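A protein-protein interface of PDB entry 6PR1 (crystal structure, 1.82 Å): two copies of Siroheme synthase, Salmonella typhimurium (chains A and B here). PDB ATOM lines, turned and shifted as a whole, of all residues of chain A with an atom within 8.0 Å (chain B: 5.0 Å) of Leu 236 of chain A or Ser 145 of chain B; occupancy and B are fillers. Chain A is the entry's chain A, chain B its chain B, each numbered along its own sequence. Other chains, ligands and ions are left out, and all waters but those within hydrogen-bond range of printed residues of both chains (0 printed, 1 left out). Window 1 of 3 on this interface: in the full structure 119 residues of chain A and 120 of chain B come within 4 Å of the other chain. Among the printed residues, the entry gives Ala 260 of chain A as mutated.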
ATOM      1  N   VAL A 221       9.913  36.098  16.345  1.00  0.00           N
ATOM      2  CA  VAL A 221       8.477  35.868  16.384  1.00  0.00           C
ATOM      3  C   VAL A 221       7.908  36.521  17.632  1.00  0.00           C
ATOM      4  O   VAL A 221       8.340  36.206  18.745  1.00  0.00           O
ATOM      5  CB  VAL A 221       8.129  34.372  16.372  1.00  0.00           C
ATOM      6  CG1 VAL A 221       6.609  34.210  16.629  1.00  0.00           C
ATOM      7  CG2 VAL A 221       8.511  33.758  15.035  1.00  0.00           C
ATOM      8  N   GLY A 222       6.905  37.379  17.442  1.00  0.00           N
ATOM      9  CA  GLY A 222       6.196  37.974  18.567  1.00  0.00           C
ATOM     10  C   GLY A 222       5.197  36.993  19.163  1.00  0.00           C
ATOM     11  O   GLY A 222       4.252  36.583  18.491  1.00  0.00           O
ATOM     12  N   ALA A 228      -2.384  32.281  24.459  1.00  0.00           N
ATOM     13  CA  ALA A 228      -1.864  31.579  23.288  1.00  0.00           C
ATOM     14  C   ALA A 228      -2.723  31.804  22.062  1.00  0.00           C
ATOM     15  O   ALA A 228      -2.231  31.682  20.935  1.00  0.00           O
ATOM     16  CB  ALA A 228      -1.762  30.079  23.557  1.00  0.00           C
ATOM     17  N   GLY A 229      -3.996  32.144  22.253  1.00  0.00           N
ATOM     18  CA  GLY A 229      -4.823  32.484  21.117  1.00  0.00           C
ATOM     19  C   GLY A 229      -4.401  33.748  20.400  1.00  0.00           C
ATOM     20  O   GLY A 229      -4.887  34.003  19.296  1.00  0.00           O
ATOM     21  N   LEU A 231      -1.250  34.403  19.477  1.00  0.00           N
ATOM     22  CA  LEU A 231      -0.201  34.146  18.492  1.00  0.00           C
ATOM     23  C   LEU A 231      -0.757  34.338  17.081  1.00  0.00           C
ATOM     24  O   LEU A 231      -1.937  34.082  16.815  1.00  0.00           O
ATOM     25  CB  LEU A 231       0.356  32.728  18.691  1.00  0.00           C
ATOM     26  CG  LEU A 231       1.601  32.344  17.888  1.00  0.00           C
ATOM     27  CD1 LEU A 231       2.793  33.234  18.248  1.00  0.00           C
ATOM     28  CD2 LEU A 231       1.937  30.863  18.130  1.00  0.00           C
ATOM     29  N   THR A 232       0.090  34.828  16.172  1.00  0.00           N
ATOM     30  CA  THR A 232      -0.356  34.946  14.793  1.00  0.00           C
ATOM     31  C   THR A 232      -0.318  33.584  14.111  1.00  0.00           C
ATOM     32  O   THR A 232       0.382  32.672  14.544  1.00  0.00           O
ATOM     33  CB  THR A 232       0.511  35.917  14.004  1.00  0.00           C
ATOM     34  OG1 THR A 232       1.883  35.494  14.078  1.00  0.00           O
ATOM     35  CG2 THR A 232       0.361  37.347  14.569  1.00  0.00           C
ATOM     36  N   LEU A 233      -1.084  33.461  13.017  1.00  0.00           N
ATOM     37  CA  LEU A 233      -1.036  32.237  12.222  1.00  0.00           C
ATOM     38  C   LEU A 233       0.376  31.984  11.692  1.00  0.00           C
ATOM     39  O   LEU A 233       0.877  30.851  11.734  1.00  0.00           O
ATOM     40  CB  LEU A 233      -2.038  32.334  11.068  1.00  0.00           C
ATOM     41  CG  LEU A 233      -3.517  32.288  11.494  1.00  0.00           C
ATOM     42  CD1 LEU A 233      -4.402  32.781  10.326  1.00  0.00           C
ATOM     43  CD2 LEU A 233      -3.913  30.868  11.932  1.00  0.00           C
ATOM     44  N   LYS A 234       1.037  33.035  11.202  1.00  0.00           N
ATOM     45  CA  LYS A 234       2.410  32.886  10.731  1.00  0.00           C
ATOM     46  C   LYS A 234       3.347  32.534  11.881  1.00  0.00           C
ATOM     47  O   LYS A 234       4.272  31.735  11.709  1.00  0.00           O
ATOM     48  CB  LYS A 234       2.869  34.166  10.033  1.00  0.00           C
ATOM     49  CG  LYS A 234       4.136  33.946   9.220  1.00  0.00           C
ATOM     50  CD  LYS A 234       4.494  35.108   8.309  1.00  0.00           C
ATOM     51  CE  LYS A 234       5.813  34.821   7.587  1.00  0.00           C
ATOM     52  NZ  LYS A 234       6.588  36.060   7.286  1.00  0.00           N
ATOM     53  N   GLY A 235       3.110  33.101  13.065  1.00  0.00           N
ATOM     54  CA  GLY A 235       3.959  32.779  14.201  1.00  0.00           C
ATOM     55  C   GLY A 235       3.825  31.333  14.610  1.00  0.00           C
ATOM     56  O   GLY A 235       4.814  30.670  14.955  1.00  0.00           O
ATOM     57  N   LEU A 236       2.598  30.814  14.574  1.00  0.00           N
ATOM     58  CA  LEU A 236       2.420  29.385  14.826  1.00  0.00           C
ATOM     59  C   LEU A 236       3.173  28.539  13.807  1.00  0.00           C
ATOM     60  O   LEU A 236       3.817  27.542  14.174  1.00  0.00           O
ATOM     61  CB  LEU A 236       0.926  29.045  14.823  1.00  0.00           C
ATOM     62  CG  LEU A 236       0.613  27.547  15.020  1.00  0.00           C
ATOM     63  CD1 LEU A 236       1.061  27.049  16.398  1.00  0.00           C
ATOM     64  CD2 LEU A 236      -0.900  27.341  14.864  1.00  0.00           C
ATOM     65  N   GLN A 237       3.073  28.891  12.519  1.00  0.00           N
ATOM     66  CA  GLN A 237       3.787  28.132  11.493  1.00  0.00           C
ATOM     67  C   GLN A 237       5.272  28.045  11.825  1.00  0.00           C
ATOM     68  O   GLN A 237       5.870  26.964  11.787  1.00  0.00           O
ATOM     69  CB  GLN A 237       3.593  28.776  10.116  1.00  0.00           C
ATOM     70  CG  GLN A 237       4.334  28.054   8.973  1.00  0.00           C
ATOM     71  CD  GLN A 237       4.228  28.775   7.635  1.00  0.00           C
ATOM     72  OE1 GLN A 237       4.361  29.998   7.557  1.00  0.00           O
ATOM     73  NE2 GLN A 237       3.997  28.012   6.570  1.00  0.00           N
ATOM     74  N   GLN A 238       5.874  29.185  12.180  1.00  0.00           N
ATOM     75  CA  GLN A 238       7.317  29.227  12.447  1.00  0.00           C
ATOM     76  C   GLN A 238       7.708  28.319  13.611  1.00  0.00           C
ATOM     77  O   GLN A 238       8.681  27.557  13.514  1.00  0.00           O
ATOM     78  CB  GLN A 238       7.749  30.669  12.734  1.00  0.00           C
ATOM     79  CG  GLN A 238       7.606  31.642  11.550  1.00  0.00           C
ATOM     80  CD  GLN A 238       8.308  31.168  10.289  1.00  0.00           C
ATOM     81  OE1 GLN A 238       9.422  30.658  10.333  1.00  0.00           O
ATOM     82  NE2 GLN A 238       7.658  31.345   9.152  1.00  0.00           N
ATOM     83  N   ILE A 239       6.980  28.385  14.731  1.00  0.00           N
ATOM     84  CA  ILE A 239       7.391  27.553  15.862  1.00  0.00           C
ATOM     85  C   ILE A 239       7.009  26.082  15.685  1.00  0.00           C
ATOM     86  O   ILE A 239       7.580  25.219  16.361  1.00  0.00           O
ATOM     87  CB  ILE A 239       6.853  28.089  17.201  1.00  0.00           C
ATOM     88  CG1 ILE A 239       5.325  28.014  17.278  1.00  0.00           C
ATOM     89  CG2 ILE A 239       7.306  29.551  17.389  1.00  0.00           C
ATOM     90  CD1 ILE A 239       4.768  28.592  18.589  1.00  0.00           C
ATOM     91  N   GLN A 240       6.079  25.760  14.788  1.00  0.00           N
ATOM     92  CA  GLN A 240       5.789  24.361  14.495  1.00  0.00           C
ATOM     93  C   GLN A 240       6.801  23.738  13.541  1.00  0.00           C
ATOM     94  O   GLN A 240       6.857  22.510  13.427  1.00  0.00           O
ATOM     95  CB  GLN A 240       4.374  24.238  13.919  1.00  0.00           C
ATOM     96  CG  GLN A 240       3.280  24.391  14.983  1.00  0.00           C
ATOM     97  CD  GLN A 240       2.927  23.081  15.647  1.00  0.00           C
ATOM     98  OE1 GLN A 240       2.678  22.087  14.966  1.00  0.00           O
ATOM     99  NE2 GLN A 240       2.901  23.068  16.987  1.00  0.00           N
ATOM    100  N   GLN A 241       7.614  24.546  12.864  1.00  0.00           N
ATOM    101  CA  GLN A 241       8.595  24.021  11.927  1.00  0.00           C
ATOM    102  C   GLN A 241      10.032  24.350  12.324  1.00  0.00           C
ATOM    103  O   GLN A 241      10.964  24.041  11.562  1.00  0.00           O
ATOM    104  CB  GLN A 241       8.295  24.545  10.518  1.00  0.00           C
ATOM    105  CG  GLN A 241       8.713  25.972  10.310  1.00  0.00           C
ATOM    106  CD  GLN A 241       8.610  26.413   8.863  1.00  0.00           C
ATOM    107  OE1 GLN A 241       7.598  26.173   8.195  1.00  0.00           O
ATOM    108  NE2 GLN A 241       9.659  27.075   8.372  1.00  0.00           N
ATOM    109  N   ALA A 242      10.243  24.939  13.497  1.00  0.00           N
ATOM    110  CA  ALA A 242      11.578  25.367  13.911  1.00  0.00           C
ATOM    111  C   ALA A 242      12.446  24.189  14.352  1.00  0.00           C
ATOM    112  O   ALA A 242      11.951  23.169  14.842  1.00  0.00           O
ATOM    113  CB  ALA A 242      11.485  26.378  15.056  1.00  0.00           C
ATOM    114  N   ILE A 255       1.993  29.408  25.198  1.00  0.00           N
ATOM    115  CA  ILE A 255       2.634  29.571  23.896  1.00  0.00           C
ATOM    116  C   ILE A 255       3.701  28.498  23.694  1.00  0.00           C
ATOM    117  O   ILE A 255       3.809  27.902  22.613  1.00  0.00           O
ATOM    118  CB  ILE A 255       3.209  30.994  23.761  1.00  0.00           C
ATOM    119  CG1 ILE A 255       2.086  32.033  23.632  1.00  0.00           C
ATOM    120  CG2 ILE A 255       4.160  31.071  22.572  1.00  0.00           C
ATOM    121  CD1 ILE A 255       1.689  32.339  22.211  1.00  0.00           C
ATOM    122  N   ASN A 257       3.668  25.583  24.708  1.00  0.00           N
ATOM    123  CA  ASN A 257       2.990  24.336  24.361  1.00  0.00           C
ATOM    124  C   ASN A 257       2.736  24.201  22.863  1.00  0.00           C
ATOM    125  O   ASN A 257       2.422  23.100  22.402  1.00  0.00           O
ATOM    126  CB  ASN A 257       1.658  24.227  25.103  1.00  0.00           C
ATOM    127  CG  ASN A 257       1.814  23.703  26.504  1.00  0.00           C
ATOM    128  OD1 ASN A 257       2.795  23.032  26.818  1.00  0.00           O
ATOM    129  ND2 ASN A 257       0.847  24.006  27.361  1.00  0.00           N
ATOM    130  N   LEU A 258       2.843  25.287  22.095  1.00  0.00           N
ATOM    131  CA  LEU A 258       2.622  25.234  20.656  1.00  0.00           C
ATOM    132  C   LEU A 258       3.911  25.035  19.874  1.00  0.00           C
ATOM    133  O   LEU A 258       3.868  24.919  18.647  1.00  0.00           O
ATOM    134  CB  LEU A 258       1.934  26.516  20.174  1.00  0.00           C
ATOM    135  CG  LEU A 258       0.512  26.705  20.701  1.00  0.00           C
ATOM    136  CD1 LEU A 258       0.036  28.121  20.430  1.00  0.00           C
ATOM    137  CD2 LEU A 258      -0.416  25.687  20.068  1.00  0.00           C
ATOM    138  N   VAL A 259       5.054  25.029  20.552  1.00  0.00           N
ATOM    139  CA  VAL A 259       6.319  24.785  19.883  1.00  0.00           C
ATOM    140  C   VAL A 259       6.395  23.312  19.500  1.00  0.00           C
ATOM    141  O   VAL A 259       5.989  22.435  20.277  1.00  0.00           O
ATOM    142  CB  VAL A 259       7.483  25.189  20.809  1.00  0.00           C
ATOM    143  CG1 VAL A 259       8.811  24.760  20.204  1.00  0.00           C
ATOM    144  CG2 VAL A 259       7.456  26.713  21.078  1.00  0.00           C
ATOM    145  N   ALA A 260       6.887  23.032  18.287  1.00  0.00           N
ATOM    146  CA  ALA A 260       7.045  21.651  17.830  1.00  0.00           C
ATOM    147  C   ALA A 260       7.733  20.813  18.894  1.00  0.00           C
ATOM    148  O   ALA A 260       8.707  21.245  19.507  1.00  0.00           O
ATOM    149  CB  ALA A 260       7.862  21.588  16.538  1.00  0.00           C
ATOM    150  N   VAL A 297      14.151  30.088  15.717  1.00  0.00           N
ATOM    151  CA  VAL A 297      13.143  31.075  16.062  1.00  0.00           C
ATOM    152  C   VAL A 297      13.543  31.722  17.377  1.00  0.00           C
ATOM    153  O   VAL A 297      13.808  31.024  18.362  1.00  0.00           O
ATOM    154  CB  VAL A 297      11.736  30.463  16.165  1.00  0.00           C
ATOM    155  CG1 VAL A 297      10.759  31.494  16.761  1.00  0.00           C
ATOM    156  CG2 VAL A 297      11.264  30.006  14.793  1.00  0.00           C
ATOM    157  N   LEU A 299      11.712  33.590  19.974  1.00  0.00           N
ATOM    158  CA  LEU A 299      10.332  33.817  20.385  1.00  0.00           C
ATOM    159  C   LEU A 299      10.329  34.840  21.514  1.00  0.00           C
ATOM    160  O   LEU A 299      10.937  34.601  22.564  1.00  0.00           O
ATOM    161  CB  LEU A 299       9.724  32.493  20.836  1.00  0.00           C
ATOM    162  CG  LEU A 299       8.232  32.349  21.076  1.00  0.00           C
ATOM    163  CD1 LEU A 299       7.441  32.795  19.852  1.00  0.00           C
ATOM    164  CD2 LEU A 299       7.908  30.902  21.468  1.00  0.00           C
ATOM    165  N   VAL A 327       8.208  38.304  12.439  1.00  0.00           N
ATOM    166  CA  VAL A 327       6.759  38.138  12.519  1.00  0.00           C
ATOM    167  C   VAL A 327       6.269  39.015  13.664  1.00  0.00           C
ATOM    168  O   VAL A 327       6.611  38.754  14.833  1.00  0.00           O
ATOM    169  CB  VAL A 327       6.354  36.671  12.727  1.00  0.00           C
ATOM    170  CG1 VAL A 327       4.819  36.520  12.710  1.00  0.00           C
ATOM    171  CG2 VAL A 327       6.978  35.794  11.642  1.00  0.00           C
ATOM    172  N   GLU B 141      -0.045  21.305  12.510  1.00  0.00           N
ATOM    173  CA  GLU B 141      -0.034  22.763  12.554  1.00  0.00           C
ATOM    174  C   GLU B 141      -1.403  23.344  12.213  1.00  0.00           C
ATOM    175  O   GLU B 141      -1.870  24.291  12.865  1.00  0.00           O
ATOM    176  CB  GLU B 141       1.037  23.299  11.592  1.00  0.00           C
ATOM    177  CG  GLU B 141       1.329  24.791  11.756  1.00  0.00           C
ATOM    178  CD  GLU B 141       0.253  25.677  11.156  1.00  0.00           C
ATOM    179  OE1 GLU B 141      -0.103  26.692  11.793  1.00  0.00           O
ATOM    180  OE2 GLU B 141      -0.235  25.358  10.050  1.00  0.00           O
ATOM    181  N   LYS B 142      -2.052  22.808  11.180  1.00  0.00           N
ATOM    182  CA  LYS B 142      -3.387  23.290  10.828  1.00  0.00           C
ATOM    183  C   LYS B 142      -4.378  23.051  11.961  1.00  0.00           C
ATOM    184  O   LYS B 142      -5.197  23.925  12.282  1.00  0.00           O
ATOM    185  CB  LYS B 142      -3.859  22.616   9.538  1.00  0.00           C
ATOM    186  CG  LYS B 142      -5.213  23.093   9.045  1.00  0.00           C
ATOM    187  CD  LYS B 142      -5.096  24.443   8.342  1.00  0.00           C
ATOM    188  CE  LYS B 142      -6.355  24.780   7.543  1.00  0.00           C
ATOM    189  NZ  LYS B 142      -6.359  24.102   6.210  1.00  0.00           N
ATOM    190  N   LEU B 143      -4.321  21.878  12.591  1.00  0.00           N
ATOM    191  CA  LEU B 143      -5.265  21.573  13.655  1.00  0.00           C
ATOM    192  C   LEU B 143      -5.004  22.422  14.891  1.00  0.00           C
ATOM    193  O   LEU B 143      -5.949  22.829  15.578  1.00  0.00           O
ATOM    194  CB  LEU B 143      -5.192  20.084  13.995  1.00  0.00           C
ATOM    195  CG  LEU B 143      -5.526  19.199  12.796  1.00  0.00           C
ATOM    196  CD1 LEU B 143      -5.489  17.725  13.188  1.00  0.00           C
ATOM    197  CD2 LEU B 143      -6.866  19.574  12.202  1.00  0.00           C
ATOM    198  N   GLU B 144      -3.733  22.704  15.198  1.00  0.00           N
ATOM    199  CA  GLU B 144      -3.453  23.548  16.357  1.00  0.00           C
ATOM    200  C   GLU B 144      -4.047  24.942  16.176  1.00  0.00           C
ATOM    201  O   GLU B 144      -4.514  25.550  17.146  1.00  0.00           O
ATOM    202  CB  GLU B 144      -1.944  23.635  16.612  1.00  0.00           C
ATOM    203  CG  GLU B 144      -1.304  22.335  17.090  1.00  0.00           C
ATOM    204  CD  GLU B 144      -1.513  22.019  18.587  1.00  0.00           C
ATOM    205  OE1 GLU B 144      -2.241  22.742  19.305  1.00  0.00           O
ATOM    206  OE2 GLU B 144      -0.922  21.023  19.048  1.00  0.00           O
ATOM    207  N   SER B 145      -4.067  25.454  14.941  1.00  0.00           N
ATOM    208  CA  SER B 145      -4.649  26.773  14.702  1.00  0.00           C
ATOM    209  C   SER B 145      -6.168  26.756  14.819  1.00  0.00           C
ATOM    210  O   SER B 145      -6.771  27.778  15.158  1.00  0.00           O
ATOM    211  CB  SER B 145      -4.248  27.292  13.325  1.00  0.00           C
ATOM    212  OG  SER B 145      -5.021  26.669  12.309  1.00  0.00           O
ATOM    213  N   LEU B 146      -6.802  25.617  14.547  1.00  0.00           N
ATOM    214  CA  LEU B 146      -8.260  25.529  14.485  1.00  0.00           C
ATOM    215  C   LEU B 146      -8.921  25.264  15.828  1.00  0.00           C
ATOM    216  O   LEU B 146     -10.074  25.669  16.034  1.00  0.00           O
ATOM    217  CB  LEU B 146      -8.670  24.419  13.519  1.00  0.00           C
ATOM    218  CG  LEU B 146      -8.306  24.726  12.066  1.00  0.00           C
ATOM    219  CD1 LEU B 146      -8.722  23.586  11.150  1.00  0.00           C
ATOM    220  CD2 LEU B 146      -8.942  26.038  11.635  1.00  0.00           C
ATOM    221  N   LEU B 147      -8.246  24.573  16.734  1.00  0.00           N
ATOM    222  CA  LEU B 147      -8.883  24.140  17.972  1.00  0.00           C
ATOM    223  C   LEU B 147      -8.605  25.138  19.077  1.00  0.00           C
ATOM    224  O   LEU B 147      -7.440  25.289  19.470  1.00  0.00           O
ATOM    225  CB  LEU B 147      -8.372  22.764  18.374  1.00  0.00           C
ATOM    226  CG  LEU B 147      -8.852  21.665  17.438  1.00  0.00           C
ATOM    227  CD1 LEU B 147      -8.315  20.318  17.916  1.00  0.00           C
ATOM    228  CD2 LEU B 147     -10.373  21.662  17.393  1.00  0.00           C
ATOM    229  N   LEU B 233      -4.672  33.390  16.080  1.00  0.00           N
ATOM    230  CA  LEU B 233      -5.367  32.105  16.098  1.00  0.00           C
ATOM    231  C   LEU B 233      -6.811  32.300  16.540  1.00  0.00           C
ATOM    232  O   LEU B 233      -7.746  31.800  15.908  1.00  0.00           O
ATOM    233  CB  LEU B 233      -4.656  31.113  17.036  1.00  0.00           C
ATOM    234  CG  LEU B 233      -3.146  30.890  16.911  1.00  0.00           C
ATOM    235  CD1 LEU B 233      -2.702  29.661  17.732  1.00  0.00           C
ATOM    236  CD2 LEU B 233      -2.716  30.725  15.469  1.00  0.00           C
ATOM    237  N   LEU B 236      -8.982  33.887  13.792  1.00  0.00           N
ATOM    238  CA  LEU B 236      -9.388  32.883  12.817  1.00  0.00           C
ATOM    239  C   LEU B 236     -10.511  32.013  13.368  1.00  0.00           C
ATOM    240  O   LEU B 236     -11.500  31.736  12.674  1.00  0.00           O
ATOM    241  CB  LEU B 236      -8.173  32.032  12.438  1.00  0.00           C
ATOM    242  CG  LEU B 236      -8.545  30.862  11.538  1.00  0.00           C
ATOM    243  CD1 LEU B 236      -9.097  31.385  10.205  1.00  0.00           C
ATOM    244  CD2 LEU B 236      -7.347  29.932  11.328  1.00  0.00           C
ATOM    245  N   GLN B 237     -10.375  31.568  14.616  1.00  0.00           N
ATOM    246  CA  GLN B 237     -11.407  30.720  15.196  1.00  0.00           C
ATOM    247  C   GLN B 237     -12.744  31.451  15.246  1.00  0.00           C
ATOM    248  O   GLN B 237     -13.799  30.861  14.976  1.00  0.00           O
ATOM    249  CB  GLN B 237     -10.978  30.271  16.585  1.00  0.00           C
ATOM    250  CG  GLN B 237      -9.795  29.281  16.521  1.00  0.00           C
ATOM    251  CD  GLN B 237      -8.941  29.340  17.763  1.00  0.00           C
ATOM    252  OE1 GLN B 237      -9.348  29.883  18.789  1.00  0.00           O
ATOM    253  NE2 GLN B 237      -7.748  28.761  17.685  1.00  0.00           N
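Leu 233 of chain B touches its own counterpart, Leu 233 of chain A.
Leu 233 of chain A touches Leu 236 of chain B, and with the chains exchanged Leu 236 of chain A touches Leu 233 of chain B.
3 positions are printed for both chains.
Of the 13 pairs that touch across the chains among the printed residues, 3 have their exchanged pair printed and touching as well.
Printed residues of chain B within 4 Å of Leu 236 of chain A: Glu 141, Ser 145 and Leu 233.
Printed residues of chain B within 4 Å of Leu 258 of chain A: Glu 144 (3.5 Å).
Printed residues of chain A within 4 Å of Glu 141 of chain B: Leu 236, Gln 237 and Gln 240.
Of the printed residues of chain A, Leu 236 of chain B touches Leu 233 (3.6 Å).
Printed residues of chain B within 4 Å of Leu 231 of chain A: Leu 233 (2.9 Å).
Of the printed residues of chain B, Gln 237 of chain A touches Glu 141.
Ala 242 of chain A touches none of the printed residues of chain B.
The nearest printed residue of chain A that does not touch Glu 141 of chain B is Leu 233 of chain A (4.3 Å).
The backbone NH (N) of Leu 233 of chain B lies within hydrogen-bond range of the backbone carbonyl oxygen (O) of Gly 229 of chain A (3.3 Å).
The backbone NH (N) of Leu 233 of chain B is in hydrogen-bond range of the backbone carbonyl oxygen (O) of Leu 231 of chain A, at 2.9 Å.
Hydrophobic or aromatic side chains of chain B that line the printed part of chain A: Leu 233 and Leu 236.
Among the printed residues, 13 pairs touch across the chains.
Among the printed residues, no Asp or Glu carboxylate lies within 4 Å of a Lys or Arg side-chain nitrogen of the other chain.
Among the printed residues, merely in contact across the chains: Leu 236 of chain A with Glu 141 of chain B, Leu 258 of chain A with Glu 144 of chain B, Leu 233 of chain A with Leu 236 of chain B, Leu 236 of chain A with Ser 145 of chain B, Gln 240 of chain A with Glu 141 of chain B, Leu 233 of chain A with Leu 233 of chain B, Thr 232 of chain A with Leu 233 of chain B, Ala 228 of chain A with Leu 233 of chain B, Leu 233 of chain A with Ser 145 of chain B, Leu 236 of chain A with Leu 233 of chain B and Gln 237 of chain A with Glu 141 of chain B.
The side-chain hydroxyl (OG) of Ser 145 of chain B sits at hydrogen-bond distance from the backbone carbonyl oxygen (O) of Lys 142 of chain B.
The backbone carbonyl oxygen (O) of Ser 145 of chain B is in hydrogen-bond range of the side-chain amide nitrogen (NE2) of Gln 237 of chain B (2.9 Å).
O of Leu 258 of chain A sits at hydrogen-bond distance from NE2 of Gln 240 of chain A (2.7 Å).
The side-chain hydroxyl (OG1) of Thr 232 of chain A sits at hydrogen-bond distance from the backbone NH (N) of Gly 235 of chain A, at 2.9 Å.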
